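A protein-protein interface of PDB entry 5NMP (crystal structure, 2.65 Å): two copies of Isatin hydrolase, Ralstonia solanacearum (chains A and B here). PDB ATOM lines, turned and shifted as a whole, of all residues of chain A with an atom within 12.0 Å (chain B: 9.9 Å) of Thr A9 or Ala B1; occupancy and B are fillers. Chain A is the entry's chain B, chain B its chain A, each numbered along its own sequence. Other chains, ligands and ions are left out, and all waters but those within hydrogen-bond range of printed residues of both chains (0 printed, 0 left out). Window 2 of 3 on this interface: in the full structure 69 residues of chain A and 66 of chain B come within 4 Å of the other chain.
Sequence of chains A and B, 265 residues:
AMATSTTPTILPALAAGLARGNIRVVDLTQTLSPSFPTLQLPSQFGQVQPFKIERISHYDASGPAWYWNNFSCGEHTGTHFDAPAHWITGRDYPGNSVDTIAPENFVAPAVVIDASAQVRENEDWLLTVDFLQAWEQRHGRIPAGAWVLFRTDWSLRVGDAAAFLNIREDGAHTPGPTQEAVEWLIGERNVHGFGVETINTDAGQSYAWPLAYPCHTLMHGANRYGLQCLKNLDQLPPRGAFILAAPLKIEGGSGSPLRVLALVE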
ATOM      1  N   THR A   6     -29.355 -19.985   7.389  1.00  0.00           N
ATOM      2  CA  THR A   6     -30.373 -19.423   8.271  1.00  0.00           C
ATOM      3  C   THR A   6     -29.877 -18.146   8.947  1.00  0.00           C
ATOM      4  O   THR A   6     -28.879 -17.561   8.522  1.00  0.00           O
ATOM      5  CB  THR A   6     -30.807 -20.436   9.348  1.00  0.00           C
ATOM      6  OG1 THR A   6     -29.654 -20.918  10.049  1.00  0.00           O
ATOM      7  CG2 THR A   6     -31.535 -21.611   8.711  1.00  0.00           C
ATOM      8  N   THR A   7     -30.578 -17.725   9.999  1.00  0.00           N
ATOM      9  CA  THR A   7     -30.285 -16.470  10.693  1.00  0.00           C
ATOM     10  C   THR A   7     -28.893 -16.436  11.320  1.00  0.00           C
ATOM     11  O   THR A   7     -28.624 -17.151  12.288  1.00  0.00           O
ATOM     12  CB  THR A   7     -31.318 -16.194  11.803  1.00  0.00           C
ATOM     13  OG1 THR A   7     -31.274 -17.246  12.776  1.00  0.00           O
ATOM     14  CG2 THR A   7     -32.720 -16.104  11.218  1.00  0.00           C
ATOM     15  N   PRO A   8     -28.008 -15.590  10.771  1.00  0.00           N
ATOM     16  CA  PRO A   8     -26.643 -15.440  11.282  1.00  0.00           C
ATOM     17  C   PRO A   8     -26.617 -14.627  12.571  1.00  0.00           C
ATOM     18  O   PRO A   8     -27.535 -13.845  12.817  1.00  0.00           O
ATOM     19  CB  PRO A   8     -25.930 -14.704  10.147  1.00  0.00           C
ATOM     20  CG  PRO A   8     -27.001 -13.877   9.529  1.00  0.00           C
ATOM     21  CD  PRO A   8     -28.275 -14.680   9.642  1.00  0.00           C
ATOM     22  N   THR A   9     -25.580 -14.808  13.382  1.00  0.00           N
ATOM     23  CA  THR A   9     -25.498 -14.116  14.662  1.00  0.00           C
ATOM     24  C   THR A   9     -24.148 -13.438  14.880  1.00  0.00           C
ATOM     25  O   THR A   9     -24.078 -12.335  15.423  1.00  0.00           O
ATOM     26  CB  THR A   9     -25.763 -15.083  15.833  1.00  0.00           C
ATOM     27  OG1 THR A   9     -24.932 -16.243  15.696  1.00  0.00           O
ATOM     28  CG2 THR A   9     -27.218 -15.511  15.849  1.00  0.00           C
ATOM     29  N   ILE A  10     -23.077 -14.097  14.451  1.00  0.00           N
ATOM     30  CA  ILE A  10     -21.733 -13.607  14.726  1.00  0.00           C
ATOM     31  C   ILE A  10     -21.315 -12.474  13.787  1.00  0.00           C
ATOM     32  O   ILE A  10     -20.881 -11.417  14.244  1.00  0.00           O
ATOM     33  CB  ILE A  10     -20.701 -14.747  14.645  1.00  0.00           C
ATOM     34  CG1 ILE A  10     -21.054 -15.838  15.658  1.00  0.00           C
ATOM     35  CG2 ILE A  10     -19.299 -14.222  14.909  1.00  0.00           C
ATOM     36  CD1 ILE A  10     -20.067 -16.987  15.705  1.00  0.00           C
ATOM     37  N   LEU A  11     -21.448 -12.691  12.481  1.00  0.00           N
ATOM     38  CA  LEU A  11     -21.032 -11.688  11.499  1.00  0.00           C
ATOM     39  C   LEU A  11     -21.710 -10.316  11.664  1.00  0.00           C
ATOM     40  O   LEU A  11     -21.032  -9.293  11.567  1.00  0.00           O
ATOM     41  CB  LEU A  11     -21.256 -12.212  10.078  1.00  0.00           C
ATOM     42  CG  LEU A  11     -20.285 -13.316   9.662  1.00  0.00           C
ATOM     43  CD1 LEU A  11     -20.465 -13.671   8.194  1.00  0.00           C
ATOM     44  CD2 LEU A  11     -18.850 -12.893   9.950  1.00  0.00           C
ATOM     45  N   PRO A  12     -23.038 -10.277  11.911  1.00  0.00           N
ATOM     46  CA  PRO A  12     -23.622  -8.954  12.170  1.00  0.00           C
ATOM     47  C   PRO A  12     -23.012  -8.262  13.393  1.00  0.00           C
ATOM     48  O   PRO A  12     -22.831  -7.042  13.382  1.00  0.00           O
ATOM     49  CB  PRO A  12     -25.102  -9.266  12.410  1.00  0.00           C
ATOM     50  CG  PRO A  12     -25.340 -10.525  11.677  1.00  0.00           C
ATOM     51  CD  PRO A  12     -24.080 -11.317  11.821  1.00  0.00           C
ATOM     52  N   ALA A  13     -22.698  -9.038  14.427  1.00  0.00           N
ATOM     53  CA  ALA A  13     -22.075  -8.495  15.629  1.00  0.00           C
ATOM     54  C   ALA A  13     -20.686  -7.942  15.318  1.00  0.00           C
ATOM     55  O   ALA A  13     -20.302  -6.889  15.823  1.00  0.00           O
ATOM     56  CB  ALA A  13     -21.995  -9.558  16.715  1.00  0.00           C
ATOM     57  N   LEU A  14     -19.942  -8.658  14.479  1.00  0.00           N
ATOM     58  CA  LEU A  14     -18.605  -8.235  14.080  1.00  0.00           C
ATOM     59  C   LEU A  14     -18.637  -6.909  13.328  1.00  0.00           C
ATOM     60  O   LEU A  14     -17.843  -6.009  13.602  1.00  0.00           O
ATOM     61  CB  LEU A  14     -17.942  -9.306  13.214  1.00  0.00           C
ATOM     62  CG  LEU A  14     -16.583  -8.927  12.619  1.00  0.00           C
ATOM     63  CD1 LEU A  14     -15.544  -8.745  13.717  1.00  0.00           C
ATOM     64  CD2 LEU A  14     -16.127  -9.964  11.605  1.00  0.00           C
ATOM     65  N   ALA A  15     -19.555  -6.797  12.373  1.00  0.00           N
ATOM     66  CA  ALA A  15     -19.692  -5.576  11.589  1.00  0.00           C
ATOM     67  C   ALA A  15     -20.081  -4.405  12.484  1.00  0.00           C
ATOM     68  O   ALA A  15     -19.530  -3.311  12.365  1.00  0.00           O
ATOM     69  CB  ALA A  15     -20.719  -5.766  10.485  1.00  0.00           C
ATOM     70  N   ALA A  16     -21.027  -4.652  13.383  1.00  0.00           N
ATOM     71  CA  ALA A  16     -21.494  -3.631  14.311  1.00  0.00           C
ATOM     72  C   ALA A  16     -20.380  -3.174  15.250  1.00  0.00           C
ATOM     73  O   ALA A  16     -20.229  -1.980  15.513  1.00  0.00           O
ATOM     74  CB  ALA A  16     -22.677  -4.150  15.107  1.00  0.00           C
ATOM     75  N   GLY A  17     -19.604  -4.130  15.750  1.00  0.00           N
ATOM     76  CA  GLY A  17     -18.512  -3.835  16.661  1.00  0.00           C
ATOM     77  C   GLY A  17     -17.426  -2.997  16.018  1.00  0.00           C
ATOM     78  O   GLY A  17     -16.852  -2.114  16.656  1.00  0.00           O
ATOM     79  N   LEU A  18     -17.143  -3.278  14.749  1.00  0.00           N
ATOM     80  CA  LEU A  18     -16.169  -2.506  13.987  1.00  0.00           C
ATOM     81  C   LEU A  18     -16.682  -1.098  13.715  1.00  0.00           C
ATOM     82  O   LEU A  18     -15.918  -0.134  13.738  1.00  0.00           O
ATOM     83  CB  LEU A  18     -15.835  -3.207  12.668  1.00  0.00           C
ATOM     84  CG  LEU A  18     -14.967  -4.462  12.773  1.00  0.00           C
ATOM     85  CD1 LEU A  18     -14.981  -5.236  11.465  1.00  0.00           C
ATOM     86  CD2 LEU A  18     -13.544  -4.096  13.163  1.00  0.00           C
ATOM     87  N   ARG A  20     -18.981   0.609  15.540  1.00  0.00           N
ATOM     88  CA  ARG A  20     -19.139   1.375  16.773  1.00  0.00           C
ATOM     89  C   ARG A  20     -17.801   1.703  17.432  1.00  0.00           C
ATOM     90  O   ARG A  20     -17.700   2.664  18.196  1.00  0.00           O
ATOM     91  CB  ARG A  20     -20.031   0.624  17.762  1.00  0.00           C
ATOM     92  CG  ARG A  20     -21.500   0.582  17.370  1.00  0.00           C
ATOM     93  CD  ARG A  20     -22.356   0.050  18.509  1.00  0.00           C
ATOM     94  NE  ARG A  20     -21.977  -1.308  18.885  1.00  0.00           N
ATOM     95  CZ  ARG A  20     -22.621  -2.402  18.488  1.00  0.00           C
ATOM     96  NH1 ARG A  20     -23.687  -2.297  17.705  1.00  0.00           N
ATOM     97  NH2 ARG A  20     -22.203  -3.599  18.878  1.00  0.00           N
ATOM     98  N   ILE A  23     -14.413  -2.871  18.355  1.00  0.00           N
ATOM     99  CA  ILE A  23     -13.352  -3.661  17.750  1.00  0.00           C
ATOM    100  C   ILE A  23     -12.434  -2.764  16.929  1.00  0.00           C
ATOM    101  O   ILE A  23     -12.889  -2.042  16.041  1.00  0.00           O
ATOM    102  CB  ILE A  23     -13.918  -4.774  16.849  1.00  0.00           C
ATOM    103  CG1 ILE A  23     -14.996  -5.562  17.595  1.00  0.00           C
ATOM    104  CG2 ILE A  23     -12.803  -5.692  16.371  1.00  0.00           C
ATOM    105  CD1 ILE A  23     -15.706  -6.583  16.740  1.00  0.00           C
ATOM    106  N   GLU A 265     -10.037  -6.308  20.638  1.00  0.00           N
ATOM    107  CA  GLU A 265     -11.144  -5.770  21.417  1.00  0.00           C
ATOM    108  C   GLU A 265     -10.862  -5.864  22.912  1.00  0.00           C
ATOM    109  O   GLU A 265     -10.905  -4.861  23.626  1.00  0.00           O
ATOM    110  CB  GLU A 265     -12.443  -6.498  21.076  1.00  0.00           C
ATOM    111  CG  GLU A 265     -12.383  -7.995  21.280  1.00  0.00           C
ATOM    112  CD  GLU A 265     -13.699  -8.670  20.971  1.00  0.00           C
ATOM    113  OE1 GLU A 265     -14.710  -7.958  20.789  1.00  0.00           O
ATOM    114  OE2 GLU A 265     -13.724  -9.915  20.912  1.00  0.00           O
ATOM    115  N   ALA B   1     -23.186 -18.851  18.018  1.00  0.00           N
ATOM    116  CA  ALA B   1     -22.814 -19.358  19.338  1.00  0.00           C
ATOM    117  C   ALA B   1     -21.962 -18.344  20.097  1.00  0.00           C
ATOM    118  O   ALA B   1     -20.775 -18.180  19.806  1.00  0.00           O
ATOM    119  CB  ALA B   1     -22.075 -20.683  19.211  1.00  0.00           C
ATOM    120  N   MET B   2     -22.570 -17.672  21.071  1.00  0.00           N
ATOM    121  CA  MET B   2     -21.899 -16.597  21.800  1.00  0.00           C
ATOM    122  C   MET B   2     -22.019 -16.741  23.320  1.00  0.00           C
ATOM    123  O   MET B   2     -22.714 -17.626  23.821  1.00  0.00           O
ATOM    124  CB  MET B   2     -22.459 -15.240  21.364  1.00  0.00           C
ATOM    125  CG  MET B   2     -22.390 -14.995  19.866  1.00  0.00           C
ATOM    126  SD  MET B   2     -23.226 -13.478  19.374  1.00  0.00           S
ATOM    127  CE  MET B   2     -22.243 -12.261  20.257  1.00  0.00           C
ATOM    128  N   ALA B   3     -21.340 -15.850  24.040  1.00  0.00           N
ATOM    129  CA  ALA B   3     -21.280 -15.894  25.499  1.00  0.00           C
ATOM    130  C   ALA B   3     -22.615 -15.538  26.152  1.00  0.00           C
ATOM    131  O   ALA B   3     -23.602 -15.277  25.468  1.00  0.00           O
ATOM    132  CB  ALA B   3     -20.190 -14.962  26.000  1.00  0.00           C
ATOM    133  N   THR B   4     -22.637 -15.523  27.481  1.00  0.00           N
ATOM    134  CA  THR B   4     -23.864 -15.236  28.215  1.00  0.00           C
ATOM    135  C   THR B   4     -23.791 -13.927  29.001  1.00  0.00           C
ATOM    136  O   THR B   4     -24.182 -13.876  30.167  1.00  0.00           O
ATOM    137  CB  THR B   4     -24.218 -16.378  29.194  1.00  0.00           C
ATOM    138  OG1 THR B   4     -23.137 -16.580  30.111  1.00  0.00           O
ATOM    139  CG2 THR B   4     -24.484 -17.669  28.439  1.00  0.00           C
ATOM    140  N   PRO B   8     -21.076  -9.045  25.134  1.00  0.00           N
ATOM    141  CA  PRO B   8     -19.822  -9.801  25.227  1.00  0.00           C
ATOM    142  C   PRO B   8     -18.783  -9.399  24.185  1.00  0.00           C
ATOM    143  O   PRO B   8     -18.979  -8.442  23.437  1.00  0.00           O
ATOM    144  CB  PRO B   8     -20.274 -11.244  24.993  1.00  0.00           C
ATOM    145  CG  PRO B   8     -21.445 -11.108  24.080  1.00  0.00           C
ATOM    146  CD  PRO B   8     -22.143  -9.829  24.486  1.00  0.00           C
ATOM    147  N   THR B   9     -17.679 -10.137  24.154  1.00  0.00           N
ATOM    148  CA  THR B   9     -16.660  -9.957  23.130  1.00  0.00           C
ATOM    149  C   THR B   9     -16.945 -10.909  21.970  1.00  0.00           C
ATOM    150  O   THR B   9     -17.462 -12.008  22.173  1.00  0.00           O
ATOM    151  CB  THR B   9     -15.240 -10.198  23.688  1.00  0.00           C
ATOM    152  OG1 THR B   9     -15.212 -11.421  24.432  1.00  0.00           O
ATOM    153  CG2 THR B   9     -14.823  -9.055  24.598  1.00  0.00           C
ATOM    154  N   ILE B  10     -16.605 -10.485  20.759  1.00  0.00           N
ATOM    155  CA  ILE B  10     -17.028 -11.191  19.555  1.00  0.00           C
ATOM    156  C   ILE B  10     -15.936 -12.073  18.949  1.00  0.00           C
ATOM    157  O   ILE B  10     -16.222 -13.147  18.413  1.00  0.00           O
ATOM    158  CB  ILE B  10     -17.511 -10.188  18.496  1.00  0.00           C
ATOM    159  CG1 ILE B  10     -18.538  -9.243  19.120  1.00  0.00           C
ATOM    160  CG2 ILE B  10     -18.103 -10.908  17.295  1.00  0.00           C
ATOM    161  CD1 ILE B  10     -18.780  -7.993  18.322  1.00  0.00           C
ATOM    162  N   LEU B  11     -14.690 -11.625  19.045  1.00  0.00           N
ATOM    163  CA  LEU B  11     -13.564 -12.328  18.429  1.00  0.00           C
ATOM    164  C   LEU B  11     -13.341 -13.764  18.932  1.00  0.00           C
ATOM    165  O   LEU B  11     -12.969 -14.632  18.143  1.00  0.00           O
ATOM    166  CB  LEU B  11     -12.283 -11.514  18.609  1.00  0.00           C
ATOM    167  CG  LEU B  11     -12.303 -10.139  17.938  1.00  0.00           C
ATOM    168  CD1 LEU B  11     -10.969  -9.439  18.106  1.00  0.00           C
ATOM    169  CD2 LEU B  11     -12.663 -10.266  16.467  1.00  0.00           C
ATOM    170  N   PRO B  12     -13.546 -14.026  20.238  1.00  0.00           N
ATOM    171  CA  PRO B  12     -13.492 -15.444  20.615  1.00  0.00           C
ATOM    172  C   PRO B  12     -14.585 -16.278  19.939  1.00  0.00           C
ATOM    173  O   PRO B  12     -14.325 -17.405  19.518  1.00  0.00           O
ATOM    174  CB  PRO B  12     -13.694 -15.411  22.133  1.00  0.00           C
ATOM    175  CG  PRO B  12     -13.178 -14.087  22.541  1.00  0.00           C
ATOM    176  CD  PRO B  12     -13.555 -13.153  21.425  1.00  0.00           C
ATOM    177  N   ALA B  13     -15.789 -15.722  19.837  1.00  0.00           N
ATOM    178  CA  ALA B  13     -16.896 -16.418  19.193  1.00  0.00           C
ATOM    179  C   ALA B  13     -16.631 -16.594  17.701  1.00  0.00           C
ATOM    180  O   ALA B  13     -16.986 -17.618  17.113  1.00  0.00           O
ATOM    181  CB  ALA B  13     -18.198 -15.667  19.418  1.00  0.00           C
ATOM    182  N   LEU B  14     -16.002 -15.588  17.100  1.00  0.00           N
ATOM    183  CA  LEU B  14     -15.668 -15.611  15.680  1.00  0.00           C
ATOM    184  C   LEU B  14     -14.675 -16.720  15.355  1.00  0.00           C
ATOM    185  O   LEU B  14     -14.871 -17.486  14.410  1.00  0.00           O
ATOM    186  CB  LEU B  14     -15.097 -14.258  15.248  1.00  0.00           C
ATOM    187  CG  LEU B  14     -14.486 -14.174  13.847  1.00  0.00           C
ATOM    188  CD1 LEU B  14     -15.538 -14.406  12.776  1.00  0.00           C
ATOM    189  CD2 LEU B  14     -13.798 -12.833  13.647  1.00  0.00           C
ATOM    190  N   ALA B  15     -13.609 -16.796  16.147  1.00  0.00           N
ATOM    191  CA  ALA B  15     -12.565 -17.794  15.955  1.00  0.00           C
ATOM    192  C   ALA B  15     -13.110 -19.214  16.089  1.00  0.00           C
ATOM    193  O   ALA B  15     -12.723 -20.113  15.341  1.00  0.00           O
ATOM    194  CB  ALA B  15     -11.436 -17.565  16.947  1.00  0.00           C
ATOM    195  N   ALA B  16     -14.011 -19.409  17.046  1.00  0.00           N
ATOM    196  CA  ALA B  16     -14.595 -20.723  17.284  1.00  0.00           C
ATOM    197  C   ALA B  16     -15.548 -21.101  16.156  1.00  0.00           C
ATOM    198  O   ALA B  16     -15.625 -22.267  15.766  1.00  0.00           O
ATOM    199  CB  ALA B  16     -15.314 -20.752  18.622  1.00  0.00           C
ATOM    200  N   GLY B  17     -16.268 -20.109  15.639  1.00  0.00           N
ATOM    201  CA  GLY B  17     -17.188 -20.323  14.536  1.00  0.00           C
ATOM    202  C   GLY B  17     -16.480 -20.790  13.279  1.00  0.00           C
ATOM    203  O   GLY B  17     -16.916 -21.741  12.627  1.00  0.00           O
ATOM    204  N   LEU B  18     -15.382 -20.121  12.940  1.00  0.00           N
ATOM    205  CA  LEU B  18     -14.589 -20.490  11.772  1.00  0.00           C
ATOM    206  C   LEU B  18     -13.982 -21.882  11.936  1.00  0.00           C
ATOM    207  O   LEU B  18     -13.863 -22.633  10.967  1.00  0.00           O
ATOM    208  CB  LEU B  18     -13.489 -19.456  11.525  1.00  0.00           C
ATOM    209  CG  LEU B  18     -13.956 -18.094  11.005  1.00  0.00           C
ATOM    210  CD1 LEU B  18     -12.906 -17.029  11.267  1.00  0.00           C
ATOM    211  CD2 LEU B  18     -14.280 -18.165   9.520  1.00  0.00           C
ATOM    212  N   ARG B  20     -15.283 -24.353  13.886  1.00  0.00           N
ATOM    213  CA  ARG B  20     -16.392 -25.308  13.856  1.00  0.00           C
ATOM    214  C   ARG B  20     -16.901 -25.545  12.439  1.00  0.00           C
ATOM    215  O   ARG B  20     -17.368 -26.637  12.115  1.00  0.00           O
ATOM    216  CB  ARG B  20     -17.556 -24.825  14.732  1.00  0.00           C
ATOM    217  CG  ARG B  20     -17.363 -25.029  16.220  1.00  0.00           C
ATOM    218  CD  ARG B  20     -18.634 -24.704  16.998  1.00  0.00           C
ATOM    219  NE  ARG B  20     -18.941 -23.277  16.984  1.00  0.00           N
ATOM    220  CZ  ARG B  20     -18.621 -22.429  17.960  1.00  0.00           C
ATOM    221  NH1 ARG B  20     -17.984 -22.865  19.039  1.00  0.00           N
ATOM    222  NH2 ARG B  20     -18.940 -21.144  17.857  1.00  0.00           N
ATOM    223  N   ASN B  22     -19.107 -23.178  11.214  1.00  0.00           N
ATOM    224  CA  ASN B  22     -20.303 -22.339  11.181  1.00  0.00           C
ATOM    225  C   ASN B  22     -20.131 -21.187  10.205  1.00  0.00           C
ATOM    226  O   ASN B  22     -21.075 -20.780   9.527  1.00  0.00           O
ATOM    227  CB  ASN B  22     -20.625 -21.789  12.569  1.00  0.00           C
ATOM    228  CG  ASN B  22     -20.993 -22.872  13.549  1.00  0.00           C
ATOM    229  OD1 ASN B  22     -20.596 -22.831  14.714  1.00  0.00           O
ATOM    230  ND2 ASN B  22     -21.754 -23.857  13.083  1.00  0.00           N
ATOM    231  N   ILE B  23     -18.912 -20.665  10.150  1.00  0.00           N
ATOM    232  CA  ILE B  23     -18.569 -19.591   9.235  1.00  0.00           C
ATOM    233  C   ILE B  23     -17.586 -20.106   8.192  1.00  0.00           C
ATOM    234  O   ILE B  23     -16.511 -20.604   8.534  1.00  0.00           O
ATOM    235  CB  ILE B  23     -17.962 -18.396   9.981  1.00  0.00           C
ATOM    236  CG1 ILE B  23     -18.800 -18.061  11.217  1.00  0.00           C
ATOM    237  CG2 ILE B  23     -17.840 -17.198   9.059  1.00  0.00           C
ATOM    238  CD1 ILE B  23     -18.180 -17.007  12.113  1.00  0.00           C
ATOM    239  N   GLY B 240     -25.365 -10.426   3.769  1.00  0.00           N
ATOM    240  CA  GLY B 240     -24.894 -11.054   4.988  1.00  0.00           C
ATOM    241  C   GLY B 240     -23.429 -11.442   4.950  1.00  0.00           C
ATOM    242  O   GLY B 240     -22.829 -11.713   5.989  1.00  0.00           O
ATOM    243  N   VAL B 264     -18.942 -16.207   5.245  1.00  0.00           N
ATOM    244  CA  VAL B 264     -20.353 -16.513   5.059  1.00  0.00           C
ATOM    245  C   VAL B 264     -20.892 -17.299   6.248  1.00  0.00           C
ATOM    246  O   VAL B 264     -20.295 -18.285   6.676  1.00  0.00           O
ATOM    247  CB  VAL B 264     -20.589 -17.306   3.758  1.00  0.00           C
ATOM    248  CG1 VAL B 264     -22.052 -17.678   3.618  1.00  0.00           C
ATOM    249  CG2 VAL B 264     -20.131 -16.499   2.558  1.00  0.00           C
ATOM    250  N   GLU B 265     -22.022 -16.850   6.784  1.00  0.00           N
ATOM    251  CA  GLU B 265     -22.624 -17.480   7.950  1.00  0.00           C
ATOM    252  C   GLU B 265     -24.065 -17.886   7.669  1.00  0.00           C
ATOM    253  O   GLU B 265     -24.327 -18.999   7.216  1.00  0.00           O
ATOM    254  CB  GLU B 265     -22.565 -16.537   9.154  1.00  0.00           C
ATOM    255  CG  GLU B 265     -23.127 -17.124  10.437  1.00  0.00           C
ATOM    256  CD  GLU B 265     -23.035 -16.159  11.604  1.00  0.00           C
ATOM    257  OE1 GLU B 265     -22.617 -15.001  11.387  1.00  0.00           O
ATOM    258  OE2 GLU B 265     -23.379 -16.560  12.737  1.00  0.00           O
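The backbone NH (N) of Ile B10 lies within hydrogen-bond range of the side-chain carboxylate (OE2) of Glu A265, at 2.9 Å. The backbone NH of Leu B11 lies within hydrogen-bond range of the side-chain carboxylate of Glu A265 (2.7 Å). The backbone NH (N) of Thr A9 is in hydrogen-bond range of the side-chain carboxylate (OE2) of Glu B265 (2.9 Å). The backbone NH of Ile A10 is in hydrogen-bond range of the side-chain carboxylate of Glu B265, at 3.0 Å. The side-chain carboxylate of Glu B265 lies within hydrogen-bond range of the backbone NH of Leu A11 (2.8 Å).
Of chain B, only Ala B13, Leu B14 and Glu B265 come within 4 Å of Ile A10. Printed residues of chain B within 4 Å of Ala A13: Ile B10 (3.1 Å). Leu A18 touches none of the printed residues of chain B. Printed residues of chain A within 4 Å of Ala B1: Thr A9 (3.9 Å). Of the printed residues of chain A, Thr B9 touches Glu A265. No residue of chain A comes within 4 Å of Ala B16. Arg B20 touches none of the printed residues of chain A. The nearest residue of chain B that does not touch Thr A9 is Met B2 (4.2 Å). The nearest residue of chain A that does not touch Ala B1 is Ile A10 (4.3 Å). The nearest printed residue of chain A that does not touch Leu B11 is Leu A14 (4.3 Å).
Printed residues of chain A that touch a printed residue of chain B: Pro A8, Thr A9, Ile A10, Leu A11, Pro A12, Ala A13, Ile A23 and Glu A265. Hydrophobic or aromatic side chains of chain A that line the printed part of chain B: Pro A8, Ile A10, Leu A11, Pro A12, Ala A13 and Ile A23. Printed residues of chain B that touch a printed residue of chain A: Ala B1, Thr B9, Ile B10, Leu B11, Pro B12, Ala B13, Leu B14, Gly B240 and Glu B265. Along chain B the printed residues that touch a printed residue of chain A span positions 1 to 265.
Thr A9 touches Glu B265, and with the chains exchanged Glu A265 touches Thr B9. Ile A10 touches Ala B13, and with the chains exchanged Ala A13 touches Ile B10. Ile A10 touches Leu B14, but with the chains exchanged Leu A14 does not touch Ile B10 (4.05 Å). Pro A12 touches Glu B265, and with the chains exchanged Glu A265 touches Pro B12.
O of Gly A17 sits at hydrogen-bond distance from N of Ile A23.
Among the printed residues, pairs that only touch across the chains: Pro A8 with Glu B265 (3.5 Å), Thr A9 with Ala B1 (3.9 Å), Ile A10 with Ala B13 (3.4 Å), Ile A10 with Leu B14 (3.96 Å), Leu A11 with Gly B240 (3.8 Å), Pro A12 with Glu B265 (3.99 Å), Ala A13 with Ile B10 (3.1 Å), Ile A23 with Ile B10 (3.7 Å), Glu A265 with Thr B9 (3.2 Å) and Glu A265 with Pro B12 (3.3 Å).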
